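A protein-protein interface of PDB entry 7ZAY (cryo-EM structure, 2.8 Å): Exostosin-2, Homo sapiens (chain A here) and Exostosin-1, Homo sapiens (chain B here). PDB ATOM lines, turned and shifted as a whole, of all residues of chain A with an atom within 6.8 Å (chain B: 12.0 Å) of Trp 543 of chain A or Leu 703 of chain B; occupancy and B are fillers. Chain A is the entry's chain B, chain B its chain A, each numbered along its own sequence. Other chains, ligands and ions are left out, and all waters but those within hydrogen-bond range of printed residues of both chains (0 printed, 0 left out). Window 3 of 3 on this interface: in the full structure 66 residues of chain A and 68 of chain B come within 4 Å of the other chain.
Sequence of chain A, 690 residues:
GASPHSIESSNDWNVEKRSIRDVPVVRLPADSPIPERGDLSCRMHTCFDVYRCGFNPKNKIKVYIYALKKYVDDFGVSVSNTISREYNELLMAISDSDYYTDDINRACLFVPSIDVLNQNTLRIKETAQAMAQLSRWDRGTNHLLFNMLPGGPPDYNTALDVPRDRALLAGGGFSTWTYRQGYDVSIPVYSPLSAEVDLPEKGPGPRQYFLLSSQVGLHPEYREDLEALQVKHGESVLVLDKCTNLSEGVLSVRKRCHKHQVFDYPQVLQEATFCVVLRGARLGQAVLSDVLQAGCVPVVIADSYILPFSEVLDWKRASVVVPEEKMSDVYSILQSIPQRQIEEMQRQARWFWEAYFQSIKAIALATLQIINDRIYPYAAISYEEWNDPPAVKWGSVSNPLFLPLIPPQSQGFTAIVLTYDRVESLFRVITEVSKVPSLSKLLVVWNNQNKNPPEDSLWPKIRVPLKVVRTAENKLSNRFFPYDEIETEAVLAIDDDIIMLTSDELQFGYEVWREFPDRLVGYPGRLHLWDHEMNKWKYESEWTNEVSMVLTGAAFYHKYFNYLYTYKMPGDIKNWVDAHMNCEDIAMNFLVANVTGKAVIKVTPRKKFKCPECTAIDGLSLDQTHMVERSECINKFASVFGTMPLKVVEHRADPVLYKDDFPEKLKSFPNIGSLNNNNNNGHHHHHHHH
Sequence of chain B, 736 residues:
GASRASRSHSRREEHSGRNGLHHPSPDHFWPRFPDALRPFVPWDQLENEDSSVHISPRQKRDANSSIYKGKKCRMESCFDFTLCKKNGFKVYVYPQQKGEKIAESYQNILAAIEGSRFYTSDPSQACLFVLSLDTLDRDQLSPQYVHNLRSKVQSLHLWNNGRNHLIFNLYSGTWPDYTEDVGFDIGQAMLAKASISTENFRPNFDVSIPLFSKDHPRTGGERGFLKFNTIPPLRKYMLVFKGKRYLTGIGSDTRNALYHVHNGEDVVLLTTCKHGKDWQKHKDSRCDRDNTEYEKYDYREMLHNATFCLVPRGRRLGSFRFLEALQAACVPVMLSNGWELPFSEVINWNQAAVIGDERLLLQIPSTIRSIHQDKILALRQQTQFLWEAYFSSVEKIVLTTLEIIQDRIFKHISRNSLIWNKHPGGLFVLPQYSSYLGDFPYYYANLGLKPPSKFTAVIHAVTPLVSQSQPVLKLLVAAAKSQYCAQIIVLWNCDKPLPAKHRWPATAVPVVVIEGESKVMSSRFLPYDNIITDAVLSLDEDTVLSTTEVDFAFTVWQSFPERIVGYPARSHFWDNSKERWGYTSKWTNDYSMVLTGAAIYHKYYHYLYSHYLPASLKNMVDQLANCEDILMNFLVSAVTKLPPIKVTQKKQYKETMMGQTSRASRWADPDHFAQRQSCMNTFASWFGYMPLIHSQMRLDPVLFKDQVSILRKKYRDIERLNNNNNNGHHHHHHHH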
ATOM      1  N   GLU A 540     -15.049  -2.419  24.944  1.00  0.00           N
ATOM      2  CA  GLU A 540     -14.599  -1.063  24.664  1.00  0.00           C
ATOM      3  C   GLU A 540     -15.804  -0.144  24.541  1.00  0.00           C
ATOM      4  O   GLU A 540     -16.736  -0.429  23.778  1.00  0.00           O
ATOM      5  CB  GLU A 540     -13.772  -0.993  23.378  1.00  0.00           C
ATOM      6  CG  GLU A 540     -12.271  -1.072  23.578  1.00  0.00           C
ATOM      7  CD  GLU A 540     -11.510  -0.563  22.370  1.00  0.00           C
ATOM      8  OE1 GLU A 540     -12.009   0.369  21.707  1.00  0.00           O
ATOM      9  OE2 GLU A 540     -10.409  -1.077  22.089  1.00  0.00           O
ATOM     10  N   SER A 541     -15.764   0.967  25.278  1.00  0.00           N
ATOM     11  CA  SER A 541     -16.718   2.052  25.125  1.00  0.00           C
ATOM     12  C   SER A 541     -16.073   3.348  24.662  1.00  0.00           C
ATOM     13  O   SER A 541     -16.795   4.315  24.394  1.00  0.00           O
ATOM     14  CB  SER A 541     -17.459   2.306  26.448  1.00  0.00           C
ATOM     15  OG  SER A 541     -16.549   2.632  27.484  1.00  0.00           O
ATOM     16  N   GLU A 542     -14.748   3.395  24.558  1.00  0.00           N
ATOM     17  CA  GLU A 542     -14.035   4.589  24.143  1.00  0.00           C
ATOM     18  C   GLU A 542     -14.146   4.774  22.631  1.00  0.00           C
ATOM     19  O   GLU A 542     -14.544   3.870  21.893  1.00  0.00           O
ATOM     20  CB  GLU A 542     -12.571   4.510  24.569  1.00  0.00           C
ATOM     21  CG  GLU A 542     -11.806   3.357  23.941  1.00  0.00           C
ATOM     22  CD  GLU A 542     -10.932   3.798  22.784  1.00  0.00           C
ATOM     23  OE1 GLU A 542     -10.692   5.016  22.652  1.00  0.00           O
ATOM     24  OE2 GLU A 542     -10.487   2.928  22.007  1.00  0.00           O
ATOM     25  N   TRP A 543     -13.794   5.976  22.173  1.00  0.00           N
ATOM     26  CA  TRP A 543     -13.868   6.299  20.753  1.00  0.00           C
ATOM     27  C   TRP A 543     -12.942   5.394  19.951  1.00  0.00           C
ATOM     28  O   TRP A 543     -11.715   5.491  20.059  1.00  0.00           O
ATOM     29  CB  TRP A 543     -13.511   7.768  20.513  1.00  0.00           C
ATOM     30  CG  TRP A 543     -14.163   8.720  21.475  1.00  0.00           C
ATOM     31  CD1 TRP A 543     -13.772   8.990  22.755  1.00  0.00           C
ATOM     32  CD2 TRP A 543     -15.318   9.531  21.230  1.00  0.00           C
ATOM     33  NE1 TRP A 543     -14.613   9.916  23.321  1.00  0.00           N
ATOM     34  CE2 TRP A 543     -15.571  10.265  22.406  1.00  0.00           C
ATOM     35  CE3 TRP A 543     -16.164   9.708  20.130  1.00  0.00           C
ATOM     36  CZ2 TRP A 543     -16.633  11.160  22.514  1.00  0.00           C
ATOM     37  CZ3 TRP A 543     -17.218  10.598  20.240  1.00  0.00           C
ATOM     38  CH2 TRP A 543     -17.443  11.313  21.423  1.00  0.00           C
ATOM     39  N   THR A 544     -13.525   4.515  19.141  1.00  0.00           N
ATOM     40  CA  THR A 544     -12.781   3.522  18.384  1.00  0.00           C
ATOM     41  C   THR A 544     -13.265   3.503  16.940  1.00  0.00           C
ATOM     42  O   THR A 544     -14.377   3.936  16.628  1.00  0.00           O
ATOM     43  CB  THR A 544     -12.900   2.133  19.026  1.00  0.00           C
ATOM     44  OG1 THR A 544     -12.023   1.212  18.364  1.00  0.00           O
ATOM     45  CG2 THR A 544     -14.329   1.638  18.976  1.00  0.00           C
ATOM     46  N   ASN A 545     -12.414   2.980  16.060  1.00  0.00           N
ATOM     47  CA  ASN A 545     -12.671   2.959  14.624  1.00  0.00           C
ATOM     48  C   ASN A 545     -13.636   1.863  14.184  1.00  0.00           C
ATOM     49  O   ASN A 545     -13.947   1.788  12.990  1.00  0.00           O
ATOM     50  CB  ASN A 545     -11.352   2.809  13.861  1.00  0.00           C
ATOM     51  CG  ASN A 545     -10.352   3.895  14.206  1.00  0.00           C
ATOM     52  OD1 ASN A 545      -9.670   3.824  15.228  1.00  0.00           O
ATOM     53  ND2 ASN A 545     -10.259   4.906  13.351  1.00  0.00           N
ATOM     54  N   GLU A 546     -14.110   1.013  15.090  1.00  0.00           N
ATOM     55  CA  GLU A 546     -15.029  -0.056  14.729  1.00  0.00           C
ATOM     56  C   GLU A 546     -16.197  -0.085  15.704  1.00  0.00           C
ATOM     57  O   GLU A 546     -16.092   0.366  16.845  1.00  0.00           O
ATOM     58  CB  GLU A 546     -14.330  -1.421  14.715  1.00  0.00           C
ATOM     59  CG  GLU A 546     -13.122  -1.505  13.792  1.00  0.00           C
ATOM     60  CD  GLU A 546     -11.838  -1.059  14.465  1.00  0.00           C
ATOM     61  OE1 GLU A 546     -11.835  -0.917  15.706  1.00  0.00           O
ATOM     62  OE2 GLU A 546     -10.834  -0.849  13.753  1.00  0.00           O
ATOM     63  N   VAL A 547     -17.322  -0.623  15.241  1.00  0.00           N
ATOM     64  CA  VAL A 547     -18.525  -0.743  16.053  1.00  0.00           C
ATOM     65  C   VAL A 547     -19.083  -2.148  15.890  1.00  0.00           C
ATOM     66  O   VAL A 547     -19.149  -2.675  14.775  1.00  0.00           O
ATOM     67  CB  VAL A 547     -19.585   0.311  15.664  1.00  0.00           C
ATOM     68  CG1 VAL A 547     -20.884   0.069  16.414  1.00  0.00           C
ATOM     69  CG2 VAL A 547     -19.069   1.714  15.938  1.00  0.00           C
ATOM     70  N   LYS A 602     -24.998   2.282  13.521  1.00  0.00           N
ATOM     71  CA  LYS A 602     -24.849   3.331  14.516  1.00  0.00           C
ATOM     72  C   LYS A 602     -25.183   4.663  13.855  1.00  0.00           C
ATOM     73  O   LYS A 602     -24.664   4.973  12.778  1.00  0.00           O
ATOM     74  CB  LYS A 602     -23.434   3.334  15.093  1.00  0.00           C
ATOM     75  CG  LYS A 602     -23.147   4.447  16.084  1.00  0.00           C
ATOM     76  CD  LYS A 602     -22.184   5.472  15.520  1.00  0.00           C
ATOM     77  CE  LYS A 602     -21.543   6.273  16.638  1.00  0.00           C
ATOM     78  NZ  LYS A 602     -22.564   6.794  17.587  1.00  0.00           N
ATOM     79  N   PRO A 605     -22.461  10.433  15.884  1.00  0.00           N
ATOM     80  CA  PRO A 605     -21.570  10.253  17.038  1.00  0.00           C
ATOM     81  C   PRO A 605     -22.268  10.546  18.356  1.00  0.00           C
ATOM     82  O   PRO A 605     -22.480  11.714  18.700  1.00  0.00           O
ATOM     83  CB  PRO A 605     -20.437  11.254  16.770  1.00  0.00           C
ATOM     84  CG  PRO A 605     -20.512  11.545  15.305  1.00  0.00           C
ATOM     85  CD  PRO A 605     -21.966  11.473  14.966  1.00  0.00           C
ATOM     86  N   ARG A 606     -22.593   9.486  19.098  1.00  0.00           N
ATOM     87  CA  ARG A 606     -23.322   9.529  20.374  1.00  0.00           C
ATOM     88  C   ARG A 606     -24.231  10.744  20.558  1.00  0.00           C
ATOM     89  O   ARG A 606     -25.109  11.004  19.736  1.00  0.00           O
ATOM     90  CB  ARG A 606     -22.333   9.455  21.545  1.00  0.00           C
ATOM     91  CG  ARG A 606     -21.200  10.468  21.497  1.00  0.00           C
ATOM     92  CD  ARG A 606     -20.634  10.736  22.882  1.00  0.00           C
ATOM     93  NE  ARG A 606     -21.548  11.502  23.722  1.00  0.00           N
ATOM     94  CZ  ARG A 606     -21.330  11.782  24.998  1.00  0.00           C
ATOM     95  NH1 ARG A 606     -20.245  11.356  25.624  1.00  0.00           N
ATOM     96  NH2 ARG A 606     -22.224  12.506  25.666  1.00  0.00           N
ATOM     97  N   ARG A 652     -21.091   4.067   9.684  1.00  0.00           N
ATOM     98  CA  ARG A 652     -22.231   4.605  10.408  1.00  0.00           C
ATOM     99  C   ARG A 652     -23.149   5.333   9.435  1.00  0.00           C
ATOM    100  O   ARG A 652     -22.700   5.878   8.421  1.00  0.00           O
ATOM    101  CB  ARG A 652     -21.795   5.556  11.530  1.00  0.00           C
ATOM    102  CG  ARG A 652     -21.224   6.879  11.056  1.00  0.00           C
ATOM    103  CD  ARG A 652     -21.075   7.847  12.217  1.00  0.00           C
ATOM    104  NE  ARG A 652     -21.414   9.212  11.836  1.00  0.00           N
ATOM    105  CZ  ARG A 652     -20.570  10.233  11.879  1.00  0.00           C
ATOM    106  NH1 ARG A 652     -19.350  10.101  12.372  1.00  0.00           N
ATOM    107  NH2 ARG A 652     -20.971  11.425  11.445  1.00  0.00           N
ATOM    108  N   PHE B 552     -12.884   1.783   1.919  1.00  0.00           N
ATOM    109  CA  PHE B 552     -14.145   1.885   2.644  1.00  0.00           C
ATOM    110  C   PHE B 552     -15.310   1.398   1.794  1.00  0.00           C
ATOM    111  O   PHE B 552     -16.205   0.704   2.293  1.00  0.00           O
ATOM    112  CB  PHE B 552     -14.383   3.323   3.104  1.00  0.00           C
ATOM    113  CG  PHE B 552     -15.678   3.510   3.839  1.00  0.00           C
ATOM    114  CD1 PHE B 552     -15.839   3.015   5.123  1.00  0.00           C
ATOM    115  CD2 PHE B 552     -16.740   4.169   3.245  1.00  0.00           C
ATOM    116  CE1 PHE B 552     -17.030   3.179   5.802  1.00  0.00           C
ATOM    117  CE2 PHE B 552     -17.935   4.338   3.919  1.00  0.00           C
ATOM    118  CZ  PHE B 552     -18.080   3.842   5.199  1.00  0.00           C
ATOM    119  N   THR B 648     -20.179   8.055   1.949  1.00  0.00           N
ATOM    120  CA  THR B 648     -19.501   9.332   2.160  1.00  0.00           C
ATOM    121  C   THR B 648     -20.347  10.479   1.616  1.00  0.00           C
ATOM    122  O   THR B 648     -21.287  10.255   0.847  1.00  0.00           O
ATOM    123  CB  THR B 648     -18.104   9.311   1.520  1.00  0.00           C
ATOM    124  OG1 THR B 648     -17.462   8.069   1.831  1.00  0.00           O
ATOM    125  CG2 THR B 648     -17.232  10.439   2.057  1.00  0.00           C
ATOM    126  N   GLN B 649     -20.025  11.715   2.004  1.00  0.00           N
ATOM    127  CA  GLN B 649     -20.767  12.865   1.499  1.00  0.00           C
ATOM    128  C   GLN B 649     -20.446  13.123   0.029  1.00  0.00           C
ATOM    129  O   GLN B 649     -21.331  13.031  -0.831  1.00  0.00           O
ATOM    130  CB  GLN B 649     -20.503  14.092   2.386  1.00  0.00           C
ATOM    131  CG  GLN B 649     -19.069  14.612   2.440  1.00  0.00           C
ATOM    132  CD  GLN B 649     -18.920  15.822   3.341  1.00  0.00           C
ATOM    133  OE1 GLN B 649     -19.760  16.075   4.205  1.00  0.00           O
ATOM    134  NE2 GLN B 649     -17.846  16.577   3.145  1.00  0.00           N
ATOM    135  N   ARG B 698     -27.244   8.075   4.005  1.00  0.00           N
ATOM    136  CA  ARG B 698     -25.933   7.781   3.448  1.00  0.00           C
ATOM    137  C   ARG B 698     -25.194   6.831   4.400  1.00  0.00           C
ATOM    138  O   ARG B 698     -25.663   6.534   5.500  1.00  0.00           O
ATOM    139  CB  ARG B 698     -25.205   9.100   3.162  1.00  0.00           C
ATOM    140  CG  ARG B 698     -23.755   9.224   3.599  1.00  0.00           C
ATOM    141  CD  ARG B 698     -23.188  10.605   3.326  1.00  0.00           C
ATOM    142  NE  ARG B 698     -23.909  11.674   3.973  1.00  0.00           N
ATOM    143  CZ  ARG B 698     -23.647  12.970   3.897  1.00  0.00           C
ATOM    144  NH1 ARG B 698     -23.876  13.653   2.787  1.00  0.00           N
ATOM    145  NH2 ARG B 698     -23.375  13.640   5.013  1.00  0.00           N
ATOM    146  N   LEU B 699     -24.013   6.358   4.004  1.00  0.00           N
ATOM    147  CA  LEU B 699     -23.159   5.566   4.881  1.00  0.00           C
ATOM    148  C   LEU B 699     -21.800   6.240   4.986  1.00  0.00           C
ATOM    149  O   LEU B 699     -21.152   6.497   3.966  1.00  0.00           O
ATOM    150  CB  LEU B 699     -23.013   4.134   4.363  1.00  0.00           C
ATOM    151  CG  LEU B 699     -23.947   3.103   4.997  1.00  0.00           C
ATOM    152  CD1 LEU B 699     -23.613   1.706   4.508  1.00  0.00           C
ATOM    153  CD2 LEU B 699     -23.876   3.175   6.512  1.00  0.00           C
ATOM    154  N   ASP B 700     -21.371   6.524   6.209  1.00  0.00           N
ATOM    155  CA  ASP B 700     -20.128   7.234   6.451  1.00  0.00           C
ATOM    156  C   ASP B 700     -19.212   6.428   7.360  1.00  0.00           C
ATOM    157  O   ASP B 700     -19.674   5.576   8.129  1.00  0.00           O
ATOM    158  CB  ASP B 700     -20.395   8.601   7.099  1.00  0.00           C
ATOM    159  CG  ASP B 700     -20.534   9.714   6.085  1.00  0.00           C
ATOM    160  OD1 ASP B 700     -19.560   9.978   5.350  1.00  0.00           O
ATOM    161  OD2 ASP B 700     -21.616  10.334   6.033  1.00  0.00           O
ATOM    162  N   PRO B 701     -17.904   6.669   7.296  1.00  0.00           N
ATOM    163  CA  PRO B 701     -16.995   6.057   8.267  1.00  0.00           C
ATOM    164  C   PRO B 701     -17.307   6.556   9.670  1.00  0.00           C
ATOM    165  O   PRO B 701     -17.601   7.735   9.874  1.00  0.00           O
ATOM    166  CB  PRO B 701     -15.616   6.525   7.797  1.00  0.00           C
ATOM    167  CG  PRO B 701     -15.780   6.675   6.324  1.00  0.00           C
ATOM    168  CD  PRO B 701     -17.173   7.236   6.149  1.00  0.00           C
ATOM    169  N   VAL B 702     -17.269   5.639  10.638  1.00  0.00           N
ATOM    170  CA  VAL B 702     -17.445   5.996  12.043  1.00  0.00           C
ATOM    171  C   VAL B 702     -16.464   7.104  12.414  1.00  0.00           C
ATOM    172  O   VAL B 702     -15.423   7.269  11.765  1.00  0.00           O
ATOM    173  CB  VAL B 702     -17.276   4.765  12.953  1.00  0.00           C
ATOM    174  CG1 VAL B 702     -15.805   4.481  13.205  1.00  0.00           C
ATOM    175  CG2 VAL B 702     -18.029   4.959  14.261  1.00  0.00           C
ATOM    176  N   LEU B 703     -16.792   7.867  13.455  1.00  0.00           N
ATOM    177  CA  LEU B 703     -16.030   9.059  13.838  1.00  0.00           C
ATOM    178  C   LEU B 703     -15.974  10.065  12.692  1.00  0.00           C
ATOM    179  O   LEU B 703     -15.924  11.273  12.917  1.00  0.00           O
ATOM    180  CB  LEU B 703     -14.611   8.694  14.293  1.00  0.00           C
ATOM    181  CG  LEU B 703     -14.417   8.312  15.762  1.00  0.00           C
ATOM    182  CD1 LEU B 703     -14.951   9.409  16.670  1.00  0.00           C
ATOM    183  CD2 LEU B 703     -15.079   6.983  16.078  1.00  0.00           C
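Leu 703 of chain B touches Trp 543 of chain A. O of Thr 544 of chain A touches CG1 of Val 702 of chain B, at 3.7 Å. Thr 544 of chain A touches Leu 703 of chain B (O to CD2, 3.2 Å). Asn 545 of chain A touches Val 702 of chain B. CG2 of Val 547 of chain A touches CG2 of Val 702 of chain B (3.8 Å). Arg 652 of chain A touches Leu 699 of chain B (O to CD2, 3.5 Å). Arg 652 of chain A touches Pro 701 of chain B (NH1 to O, 3.9 Å). Arg 652 of chain A touches Leu 703 of chain B.
O of Asp 700 of chain B sits at hydrogen-bond distance from N of Arg 652 of chain A.
No residue of chain B comes within 4 Å of Ser 541 of chain A. No residue of chain B comes within 4 Å of Glu 542 of chain A. Of chain B, only Val 702 (3.7 Å) and Leu 703 (3.2 Å) come within 4 Å of Thr 544 of chain A. Of the printed residues of chain B, Val 547 of chain A touches Val 702 (3.8 Å). Pro 605 of chain A touches none of the printed residues of chain B. Phe 552 of chain B touches none of the printed residues of chain A. Of the printed residues of chain A, Val 702 of chain B touches Thr 544 (3.7 Å), Asn 545 (3.3 Å) and Val 547 (3.8 Å). Printed residues of chain A within 4 Å of Leu 703 of chain B: Trp 543 (3.7 Å), Thr 544 (3.2 Å) and Arg 652 (3.4 Å). The nearest residue of chain B that does not touch Trp 543 of chain A is Val 702 of chain B (7.4 Å).
OD2 of Asp 700 of chain B lies within salt-bridge range of NE of Arg 698 of chain B, 3.4 Å away. OE1 of Glu 540 of chain A lies close to OG1 of Thr 544 of chain A. The backbone NH of Thr 648 of chain B is in hydrogen-bond range of the backbone carbonyl oxygen of Leu 699 of chain B (2.7 Å). The side-chain hydroxyl (OG1) of Thr 544 of chain A is in hydrogen-bond range of the side-chain carboxylate (OE1) of Glu 546 of chain A (3.4 Å).
Of the 12 printed residues of chain A, 5 touch a printed residue of chain B. Printed residues of chain A that touch a printed residue of chain B: Trp 543, Thr 544, Asn 545, Val 547 and Arg 652. Hydrophobic or aromatic side chains of chain A that line the printed part of chain B: Trp 543 and Val 547. Hydrophobic or aromatic side chains of chain B that line the printed part of chain A: Leu 699, Val 702 and Leu 703. Among the printed residues, no Asp or Glu carboxylate lies within 4 Å of a Lys or Arg side-chain nitrogen of the other chain.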
